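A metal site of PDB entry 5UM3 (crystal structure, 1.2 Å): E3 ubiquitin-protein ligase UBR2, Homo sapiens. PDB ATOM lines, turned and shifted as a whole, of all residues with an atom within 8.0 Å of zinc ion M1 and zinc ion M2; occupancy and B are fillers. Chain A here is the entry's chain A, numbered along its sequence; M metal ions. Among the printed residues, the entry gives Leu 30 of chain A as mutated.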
ATOM      1  N   SER A   5     -14.794 -33.193  29.455  1.00  0.00           N
ATOM      2  CA  SER A   5     -14.891 -33.245  28.005  1.00  0.00           C
ATOM      3  C   SER A   5     -13.607 -32.744  27.368  1.00  0.00           C
ATOM      4  O   SER A   5     -12.801 -32.051  27.990  1.00  0.00           O
ATOM      5  CB  SER A   5     -16.100 -32.438  27.487  1.00  0.00           C
ATOM      6  OG  SER A   5     -16.008 -31.066  27.831  1.00  0.00           O
ATOM      7  N   LEU A   6     -13.421 -33.127  26.111  1.00  0.00           N
ATOM      8  CA  LEU A   6     -12.287 -32.648  25.308  1.00  0.00           C
ATOM      9  C   LEU A   6     -12.611 -31.272  24.734  1.00  0.00           C
ATOM     10  O   LEU A   6     -13.695 -31.056  24.202  1.00  0.00           O
ATOM     11  CB  LEU A   6     -12.044 -33.608  24.152  1.00  0.00           C
ATOM     12  CG  LEU A   6     -11.435 -34.965  24.468  1.00  0.00           C
ATOM     13  CD1 LEU A   6     -11.535 -35.887  23.265  1.00  0.00           C
ATOM     14  CD2 LEU A   6      -9.978 -34.820  24.880  1.00  0.00           C
ATOM     15  N   CYS A   7     -11.653 -30.360  24.822  1.00  0.00           N
ATOM     16  CA  CYS A   7     -11.806 -29.072  24.138  1.00  0.00           C
ATOM     17  C   CYS A   7     -11.838 -29.272  22.623  1.00  0.00           C
ATOM     18  O   CYS A   7     -12.809 -28.900  21.956  1.00  0.00           O
ATOM     19  CB  CYS A   7     -10.661 -28.146  24.505  1.00  0.00           C
ATOM     20  SG  CYS A   7     -10.704 -26.594  23.564  1.00  0.00           S
ATOM     21  N   GLY A   8     -10.800 -29.881  22.075  1.00  0.00           N
ATOM     22  CA  GLY A   8     -10.717 -30.178  20.668  1.00  0.00           C
ATOM     23  C   GLY A   8     -10.604 -28.985  19.746  1.00  0.00           C
ATOM     24  O   GLY A   8     -10.718 -29.169  18.534  1.00  0.00           O
ATOM     25  N   ARG A   9     -10.368 -27.781  20.250  1.00  0.00           N
ATOM     26  CA  ARG A   9     -10.324 -26.595  19.384  1.00  0.00           C
ATOM     27  C   ARG A   9      -9.216 -26.752  18.353  1.00  0.00           C
ATOM     28  O   ARG A   9      -8.065 -27.027  18.695  1.00  0.00           O
ATOM     29  CB  ARG A   9     -10.105 -25.330  20.205  1.00  0.00           C
ATOM     30  CG  ARG A   9     -10.113 -24.058  19.350  1.00  0.00           C
ATOM     31  CD  ARG A   9     -10.220 -22.798  20.190  1.00  0.00           C
ATOM     32  NE  ARG A   9     -10.417 -21.606  19.366  1.00  0.00           N
ATOM     33  CZ  ARG A   9     -11.085 -20.523  19.738  1.00  0.00           C
ATOM     34  NH1 ARG A   9     -11.654 -20.443  20.937  1.00  0.00           N
ATOM     35  NH2 ARG A   9     -11.209 -19.500  18.899  1.00  0.00           N
ATOM     36  N   VAL A  10      -9.563 -26.556  17.087  1.00  0.00           N
ATOM     37  CA  VAL A  10      -8.608 -26.659  15.991  1.00  0.00           C
ATOM     38  C   VAL A  10      -7.907 -25.320  15.843  1.00  0.00           C
ATOM     39  O   VAL A  10      -8.559 -24.292  15.666  1.00  0.00           O
ATOM     40  CB  VAL A  10      -9.324 -27.056  14.693  1.00  0.00           C
ATOM     41  CG1 VAL A  10      -8.345 -27.037  13.549  1.00  0.00           C
ATOM     42  CG2 VAL A  10      -9.943 -28.432  14.830  1.00  0.00           C
ATOM     43  N   PHE A  11      -6.575 -25.341  15.931  1.00  0.00           N
ATOM     44  CA  PHE A  11      -5.823 -24.096  15.855  1.00  0.00           C
ATOM     45  C   PHE A  11      -5.835 -23.529  14.453  1.00  0.00           C
ATOM     46  O   PHE A  11      -5.689 -24.250  13.471  1.00  0.00           O
ATOM     47  CB  PHE A  11      -4.381 -24.313  16.299  1.00  0.00           C
ATOM     48  CG  PHE A  11      -4.241 -24.665  17.743  1.00  0.00           C
ATOM     49  CD1 PHE A  11      -4.709 -23.794  18.719  1.00  0.00           C
ATOM     50  CD2 PHE A  11      -3.645 -25.851  18.142  1.00  0.00           C
ATOM     51  CE1 PHE A  11      -4.581 -24.120  20.051  1.00  0.00           C
ATOM     52  CE2 PHE A  11      -3.513 -26.149  19.480  1.00  0.00           C
ATOM     53  CZ  PHE A  11      -3.978 -25.299  20.421  1.00  0.00           C
ATOM     54  N   LEU A  30      -0.539 -29.399  23.613  1.00  0.00           N
ATOM     55  CA  LEU A  30      -0.792 -27.959  23.514  1.00  0.00           C
ATOM     56  C   LEU A  30      -2.158 -27.631  24.087  1.00  0.00           C
ATOM     57  O   LEU A  30      -3.071 -28.454  24.084  1.00  0.00           O
ATOM     58  CB  LEU A  30      -0.734 -27.498  22.059  1.00  0.00           C
ATOM     59  CG  LEU A  30       0.641 -27.664  21.403  1.00  0.00           C
ATOM     60  CD1 LEU A  30       0.529 -27.424  19.896  1.00  0.00           C
ATOM     61  CD2 LEU A  30       1.691 -26.742  22.043  1.00  0.00           C
ATOM     62  N   LEU A  31      -2.288 -26.383  24.560  1.00  0.00           N
ATOM     63  CA  LEU A  31      -3.551 -25.820  25.013  1.00  0.00           C
ATOM     64  C   LEU A  31      -3.875 -24.540  24.257  1.00  0.00           C
ATOM     65  O   LEU A  31      -2.981 -23.766  23.916  1.00  0.00           O
ATOM     66  CB  LEU A  31      -3.477 -25.475  26.489  1.00  0.00           C
ATOM     67  CG  LEU A  31      -3.231 -26.664  27.410  1.00  0.00           C
ATOM     68  CD1 LEU A  31      -2.897 -26.208  28.814  1.00  0.00           C
ATOM     69  CD2 LEU A  31      -4.453 -27.580  27.439  1.00  0.00           C
ATOM     70  N   CYS A  32      -5.165 -24.337  24.002  1.00  0.00           N
ATOM     71  CA  CYS A  32      -5.623 -23.041  23.514  1.00  0.00           C
ATOM     72  C   CYS A  32      -5.566 -22.008  24.631  1.00  0.00           C
ATOM     73  O   CYS A  32      -5.449 -22.330  25.823  1.00  0.00           O
ATOM     74  CB  CYS A  32      -7.033 -23.138  22.935  1.00  0.00           C
ATOM     75  SG  CYS A  32      -8.360 -23.393  24.141  1.00  0.00           S
ATOM     76  N   MET A  33      -5.675 -20.737  24.248  1.00  0.00           N
ATOM     77  CA  MET A  33      -5.514 -19.664  25.229  1.00  0.00           C
ATOM     78  C   MET A  33      -6.564 -19.756  26.328  1.00  0.00           C
ATOM     79  O   MET A  33      -6.240 -19.602  27.518  1.00  0.00           O
ATOM     80  CB  MET A  33      -5.584 -18.313  24.517  1.00  0.00           C
ATOM     81  CG  MET A  33      -5.021 -17.141  25.319  1.00  0.00           C
ATOM     82  SD  MET A  33      -4.916 -15.607  24.396  1.00  0.00           S
ATOM     83  CE  MET A  33      -6.633 -15.251  24.515  1.00  0.00           C
ATOM     84  N   GLU A  34      -7.822 -20.007  25.957  1.00  0.00           N
ATOM     85  CA  GLU A  34      -8.917 -20.097  26.940  1.00  0.00           C
ATOM     86  C   GLU A  34      -8.650 -21.203  27.949  1.00  0.00           C
ATOM     87  O   GLU A  34      -8.838 -21.030  29.164  1.00  0.00           O
ATOM     88  CB  GLU A  34     -10.245 -20.344  26.194  1.00  0.00           C
ATOM     89  CG  GLU A  34     -11.477 -20.579  27.100  1.00  0.00           C
ATOM     90  CD  GLU A  34     -12.770 -20.948  26.353  1.00  0.00           C
ATOM     91  OE1 GLU A  34     -12.739 -21.690  25.340  1.00  0.00           O
ATOM     92  OE2 GLU A  34     -13.849 -20.513  26.827  1.00  0.00           O
ATOM     93  N   CYS A  35      -8.257 -22.381  27.470  1.00  0.00           N
ATOM     94  CA  CYS A  35      -7.993 -23.504  28.357  1.00  0.00           C
ATOM     95  C   CYS A  35      -6.763 -23.241  29.222  1.00  0.00           C
ATOM     96  O   CYS A  35      -6.780 -23.477  30.437  1.00  0.00           O
ATOM     97  CB  CYS A  35      -7.826 -24.771  27.540  1.00  0.00           C
ATOM     98  SG  CYS A  35      -9.433 -25.274  26.814  1.00  0.00           S
ATOM     99  N   PHE A  36      -5.692 -22.761  28.605  1.00  0.00           N
ATOM    100  CA  PHE A  36      -4.473 -22.483  29.344  1.00  0.00           C
ATOM    101  C   PHE A  36      -4.749 -21.563  30.525  1.00  0.00           C
ATOM    102  O   PHE A  36      -4.346 -21.857  31.663  1.00  0.00           O
ATOM    103  CB  PHE A  36      -3.448 -21.862  28.404  1.00  0.00           C
ATOM    104  CG  PHE A  36      -2.201 -21.409  29.087  1.00  0.00           C
ATOM    105  CD1 PHE A  36      -1.262 -22.324  29.569  1.00  0.00           C
ATOM    106  CD2 PHE A  36      -1.960 -20.052  29.282  1.00  0.00           C
ATOM    107  CE1 PHE A  36      -0.122 -21.897  30.212  1.00  0.00           C
ATOM    108  CE2 PHE A  36      -0.805 -19.614  29.930  1.00  0.00           C
ATOM    109  CZ  PHE A  36       0.106 -20.549  30.390  1.00  0.00           C
ATOM    110  N   GLY A  38      -7.440 -20.974  32.105  1.00  0.00           N
ATOM    111  CA  GLY A  38      -8.355 -21.566  33.068  1.00  0.00           C
ATOM    112  C   GLY A  38      -7.829 -22.847  33.681  1.00  0.00           C
ATOM    113  O   GLY A  38      -8.579 -23.587  34.306  1.00  0.00           O
ATOM    114  N   SER A  39      -6.515 -23.088  33.562  1.00  0.00           N
ATOM    115  CA  SER A  39      -5.884 -24.327  33.998  1.00  0.00           C
ATOM    116  C   SER A  39      -4.807 -24.016  35.030  1.00  0.00           C
ATOM    117  O   SER A  39      -4.401 -22.872  35.219  1.00  0.00           O
ATOM    118  CB  SER A  39      -5.246 -25.067  32.818  1.00  0.00           C
ATOM    119  OG  SER A  39      -4.012 -24.466  32.480  1.00  0.00           O
ATOM    120  N   PHE A  56      -4.719 -29.425  17.434  1.00  0.00           N
ATOM    121  CA  PHE A  56      -5.836 -29.023  18.283  1.00  0.00           C
ATOM    122  C   PHE A  56      -5.388 -28.935  19.727  1.00  0.00           C
ATOM    123  O   PHE A  56      -4.338 -29.451  20.134  1.00  0.00           O
ATOM    124  CB  PHE A  56      -7.034 -29.956  18.124  1.00  0.00           C
ATOM    125  CG  PHE A  56      -6.645 -31.331  17.742  1.00  0.00           C
ATOM    126  CD1 PHE A  56      -6.775 -31.769  16.440  1.00  0.00           C
ATOM    127  CD2 PHE A  56      -6.108 -32.195  18.683  1.00  0.00           C
ATOM    128  CE1 PHE A  56      -6.393 -33.039  16.083  1.00  0.00           C
ATOM    129  CE2 PHE A  56      -5.712 -33.457  18.341  1.00  0.00           C
ATOM    130  CZ  PHE A  56      -5.854 -33.890  17.028  1.00  0.00           C
ATOM    131  N   CYS A  57      -6.215 -28.238  20.494  1.00  0.00           N
ATOM    132  CA  CYS A  57      -6.057 -28.151  21.924  1.00  0.00           C
ATOM    133  C   CYS A  57      -6.237 -29.529  22.541  1.00  0.00           C
ATOM    134  O   CYS A  57      -7.169 -30.238  22.193  1.00  0.00           O
ATOM    135  CB  CYS A  57      -7.104 -27.188  22.486  1.00  0.00           C
ATOM    136  SG  CYS A  57      -7.017 -27.047  24.283  1.00  0.00           S
ATOM    137  N   ASP A  58      -5.327 -29.878  23.444  1.00  0.00           N
ATOM    138  CA  ASP A  58      -5.326 -31.166  24.124  1.00  0.00           C
ATOM    139  C   ASP A  58      -5.940 -31.098  25.521  1.00  0.00           C
ATOM    140  O   ASP A  58      -5.731 -32.029  26.308  1.00  0.00           O
ATOM    141  CB  ASP A  58      -3.893 -31.686  24.227  1.00  0.00           C
ATOM    142  CG  ASP A  58      -3.318 -32.074  22.878  1.00  0.00           C
ATOM    143  OD1 ASP A  58      -3.988 -32.819  22.137  1.00  0.00           O
ATOM    144  OD2 ASP A  58      -2.197 -31.645  22.577  1.00  0.00           O
ATOM    145  N   CYS A  59      -6.663 -30.038  25.843  1.00  0.00           N
ATOM    146  CA  CYS A  59      -7.350 -29.977  27.116  1.00  0.00           C
ATOM    147  C   CYS A  59      -8.381 -31.105  27.200  1.00  0.00           C
ATOM    148  O   CYS A  59      -9.160 -31.329  26.269  1.00  0.00           O
ATOM    149  CB  CYS A  59      -8.037 -28.630  27.296  1.00  0.00           C
ATOM    150  SG  CYS A  59      -8.727 -28.400  28.917  1.00  0.00           S
ATOM    151  N   GLY A  60      -8.364 -31.806  28.316  1.00  0.00           N
ATOM    152  CA  GLY A  60      -9.246 -32.922  28.522  1.00  0.00           C
ATOM    153  C   GLY A  60      -8.657 -34.260  28.121  1.00  0.00           C
ATOM    154  O   GLY A  60      -9.323 -35.290  28.313  1.00  0.00           O
ATOM    155  N   PRO A  69      -5.034 -32.128  33.665  1.00  0.00           N
ATOM    156  CA  PRO A  69      -5.432 -32.332  32.266  1.00  0.00           C
ATOM    157  C   PRO A  69      -6.633 -31.526  31.824  1.00  0.00           C
ATOM    158  O   PRO A  69      -6.791 -31.319  30.615  1.00  0.00           O
ATOM    159  CB  PRO A  69      -5.722 -33.835  32.193  1.00  0.00           C
ATOM    160  CG  PRO A  69      -6.068 -34.216  33.581  1.00  0.00           C
ATOM    161  CD  PRO A  69      -5.197 -33.359  34.460  1.00  0.00           C
ATOM    162  N   TYR A  70      -7.471 -31.048  32.744  1.00  0.00           N
ATOM    163  CA  TYR A  70      -8.640 -30.252  32.402  1.00  0.00           C
ATOM    164  C   TYR A  70      -8.505 -28.825  32.927  1.00  0.00           C
ATOM    165  O   TYR A  70      -7.888 -28.579  33.964  1.00  0.00           O
ATOM    166  CB  TYR A  70      -9.914 -30.819  33.035  1.00  0.00           C
ATOM    167  CG  TYR A  70     -10.360 -32.151  32.504  1.00  0.00           C
ATOM    168  CD1 TYR A  70      -9.977 -33.339  33.118  1.00  0.00           C
ATOM    169  CD2 TYR A  70     -11.210 -32.215  31.407  1.00  0.00           C
ATOM    170  CE1 TYR A  70     -10.418 -34.558  32.638  1.00  0.00           C
ATOM    171  CE2 TYR A  70     -11.666 -33.435  30.934  1.00  0.00           C
ATOM    172  CZ  TYR A  70     -11.265 -34.596  31.548  1.00  0.00           C
ATOM    173  OH  TYR A  70     -11.721 -35.789  31.060  1.00  0.00           O
ATOM    174  N   CYS A  71      -9.167 -27.913  32.244  1.00  0.00           N
ATOM    175  CA  CYS A  71      -9.336 -26.543  32.696  1.00  0.00           C
ATOM    176  C   CYS A  71     -10.722 -26.410  33.341  1.00  0.00           C
ATOM    177  O   CYS A  71     -11.524 -27.348  33.324  1.00  0.00           O
ATOM    178  CB  CYS A  71      -9.182 -25.562  31.530  1.00  0.00           C
ATOM    179  SG  CYS A  71     -10.641 -25.503  30.451  1.00  0.00           S
ATOM    180  N   GLN A  72     -11.024 -25.217  33.856  1.00  0.00           N
ATOM    181  CA  GLN A  72     -12.303 -24.995  34.527  1.00  0.00           C
ATOM    182  C   GLN A  72     -13.490 -25.183  33.586  1.00  0.00           C
ATOM    183  O   GLN A  72     -14.577 -25.561  34.034  1.00  0.00           O
ATOM    184  CB  GLN A  72     -12.333 -23.600  35.165  1.00  0.00           C
ATOM    185  CG  GLN A  72     -12.125 -22.397  34.215  1.00  0.00           C
ATOM    186  CD  GLN A  72     -13.363 -22.047  33.386  1.00  0.00           C
ATOM    187  OE1 GLN A  72     -14.510 -22.169  33.822  1.00  0.00           O
ATOM    188  NE2 GLN A  72     -13.135 -21.581  32.172  1.00  0.00           N
ATOM    189  N   LYS A  73     -13.322 -24.928  32.283  1.00  0.00           N
ATOM    190  CA  LYS A  73     -14.444 -25.070  31.358  1.00  0.00           C
ATOM    191  C   LYS A  73     -14.754 -26.533  31.069  1.00  0.00           C
ATOM    192  O   LYS A  73     -15.927 -26.914  30.937  1.00  0.00           O
ATOM    193  CB  LYS A  73     -14.143 -24.342  30.046  1.00  0.00           C
ATOM    194  CG  LYS A  73     -15.279 -24.401  29.043  1.00  0.00           C
ATOM    195  CD  LYS A  73     -14.923 -23.710  27.756  1.00  0.00           C
ATOM    196  CE  LYS A  73     -16.127 -23.651  26.840  1.00  0.00           C
ATOM    197  NZ  LYS A  73     -15.805 -23.068  25.508  1.00  0.00           N
ATOM    198  N   HIS A  74     -13.713 -27.363  30.962  1.00  0.00           N
ATOM    199  CA  HIS A  74     -13.884 -28.704  30.439  1.00  0.00           C
ATOM    200  C   HIS A  74     -13.908 -29.803  31.489  1.00  0.00           C
ATOM    201  O   HIS A  74     -14.278 -30.933  31.153  1.00  0.00           O
ATOM    202  CB  HIS A  74     -12.828 -28.971  29.378  1.00  0.00           C
ATOM    203  CG  HIS A  74     -13.025 -28.110  28.176  1.00  0.00           C
ATOM    204  ND1 HIS A  74     -12.129 -27.131  27.792  1.00  0.00           N
ATOM    205  CD2 HIS A  74     -14.059 -28.030  27.315  1.00  0.00           C
ATOM    206  CE1 HIS A  74     -12.609 -26.503  26.741  1.00  0.00           C
ATOM    207  NE2 HIS A  74     -13.775 -27.037  26.414  1.00  0.00           N
ATOM    208  N   GLU A  75     -13.558 -29.497  32.733  1.00  0.00           N
ATOM    209  CA  GLU A  75     -13.582 -30.534  33.767  1.00  0.00           C
ATOM    210  C   GLU A  75     -15.004 -30.971  34.061  1.00  0.00           C
ATOM    211  O   GLU A  75     -15.165 -32.056  34.597  1.00  0.00           O
ATOM    212  CB  GLU A  75     -12.924 -30.054  35.062  1.00  0.00           C
ATOM    213  CG  GLU A  75     -13.659 -28.923  35.768  1.00  0.00           C
ATOM    214  CD  GLU A  75     -12.950 -28.427  37.005  1.00  0.00           C
ATOM    215  OE1 GLU A  75     -12.135 -29.168  37.586  1.00  0.00           O
ATOM    216  OE2 GLU A  75     -13.211 -27.268  37.383  1.00  0.00           O
ATOM    217  OXT GLU A  75     -15.969 -30.265  33.784  1.00  0.00           O
HETATM  218 ZN    ZN M   1     -10.229 -26.710  28.511  1.00  0.00          ZN
HETATM  219 ZN    ZN M   2      -8.859 -25.636  24.532  1.00  0.00          ZN
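O of His 74 is in hydrogen-bond range of N of Ser 5 (2.9 Å).
O of Cys 59 lies within hydrogen-bond range of N of Cys 7, 3.0 Å away.
The side-chain sulfur (SG) of Cys 7 lies close to the backbone NH (N) of Arg 9 (3.5 Å).
The side-chain sulfur (SG) of Cys 57 lies close to the backbone NH (N) of Cys 59 (3.4 Å).
The backbone NH (N) of Lys 73 lies close to the side-chain sulfur (SG) of Cys 71.
N of Cys 57 sits at hydrogen-bond distance from O of Arg 9, at 2.9 Å.
Within 4 Å of zinc ion M1: Cys 35, Cys 59, Cys 71 and His 74.
Along chain A the residues within 4 Å of zinc ion M1 span positions 35 to 74.
Zinc ion M1 is bound by ND1 of His 74 (2.1 Å), SG of Cys 59 (2.3 Å), SG of Cys 71 (2.3 Å) and SG of Cys 35 (2.4 Å).
Of the 28 residues printed, 4 come within 4 Å of zinc ion M2.
The nearest printed residue that does not touch zinc ion M2 is Cys 59 (4.2 Å).
Zinc ion M2 is bound by SG of Cys 7, SG of Cys 32, SG of Cys 57 and SG of Cys 35.
Zinc ion M2 has four donor atoms within binding distance.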
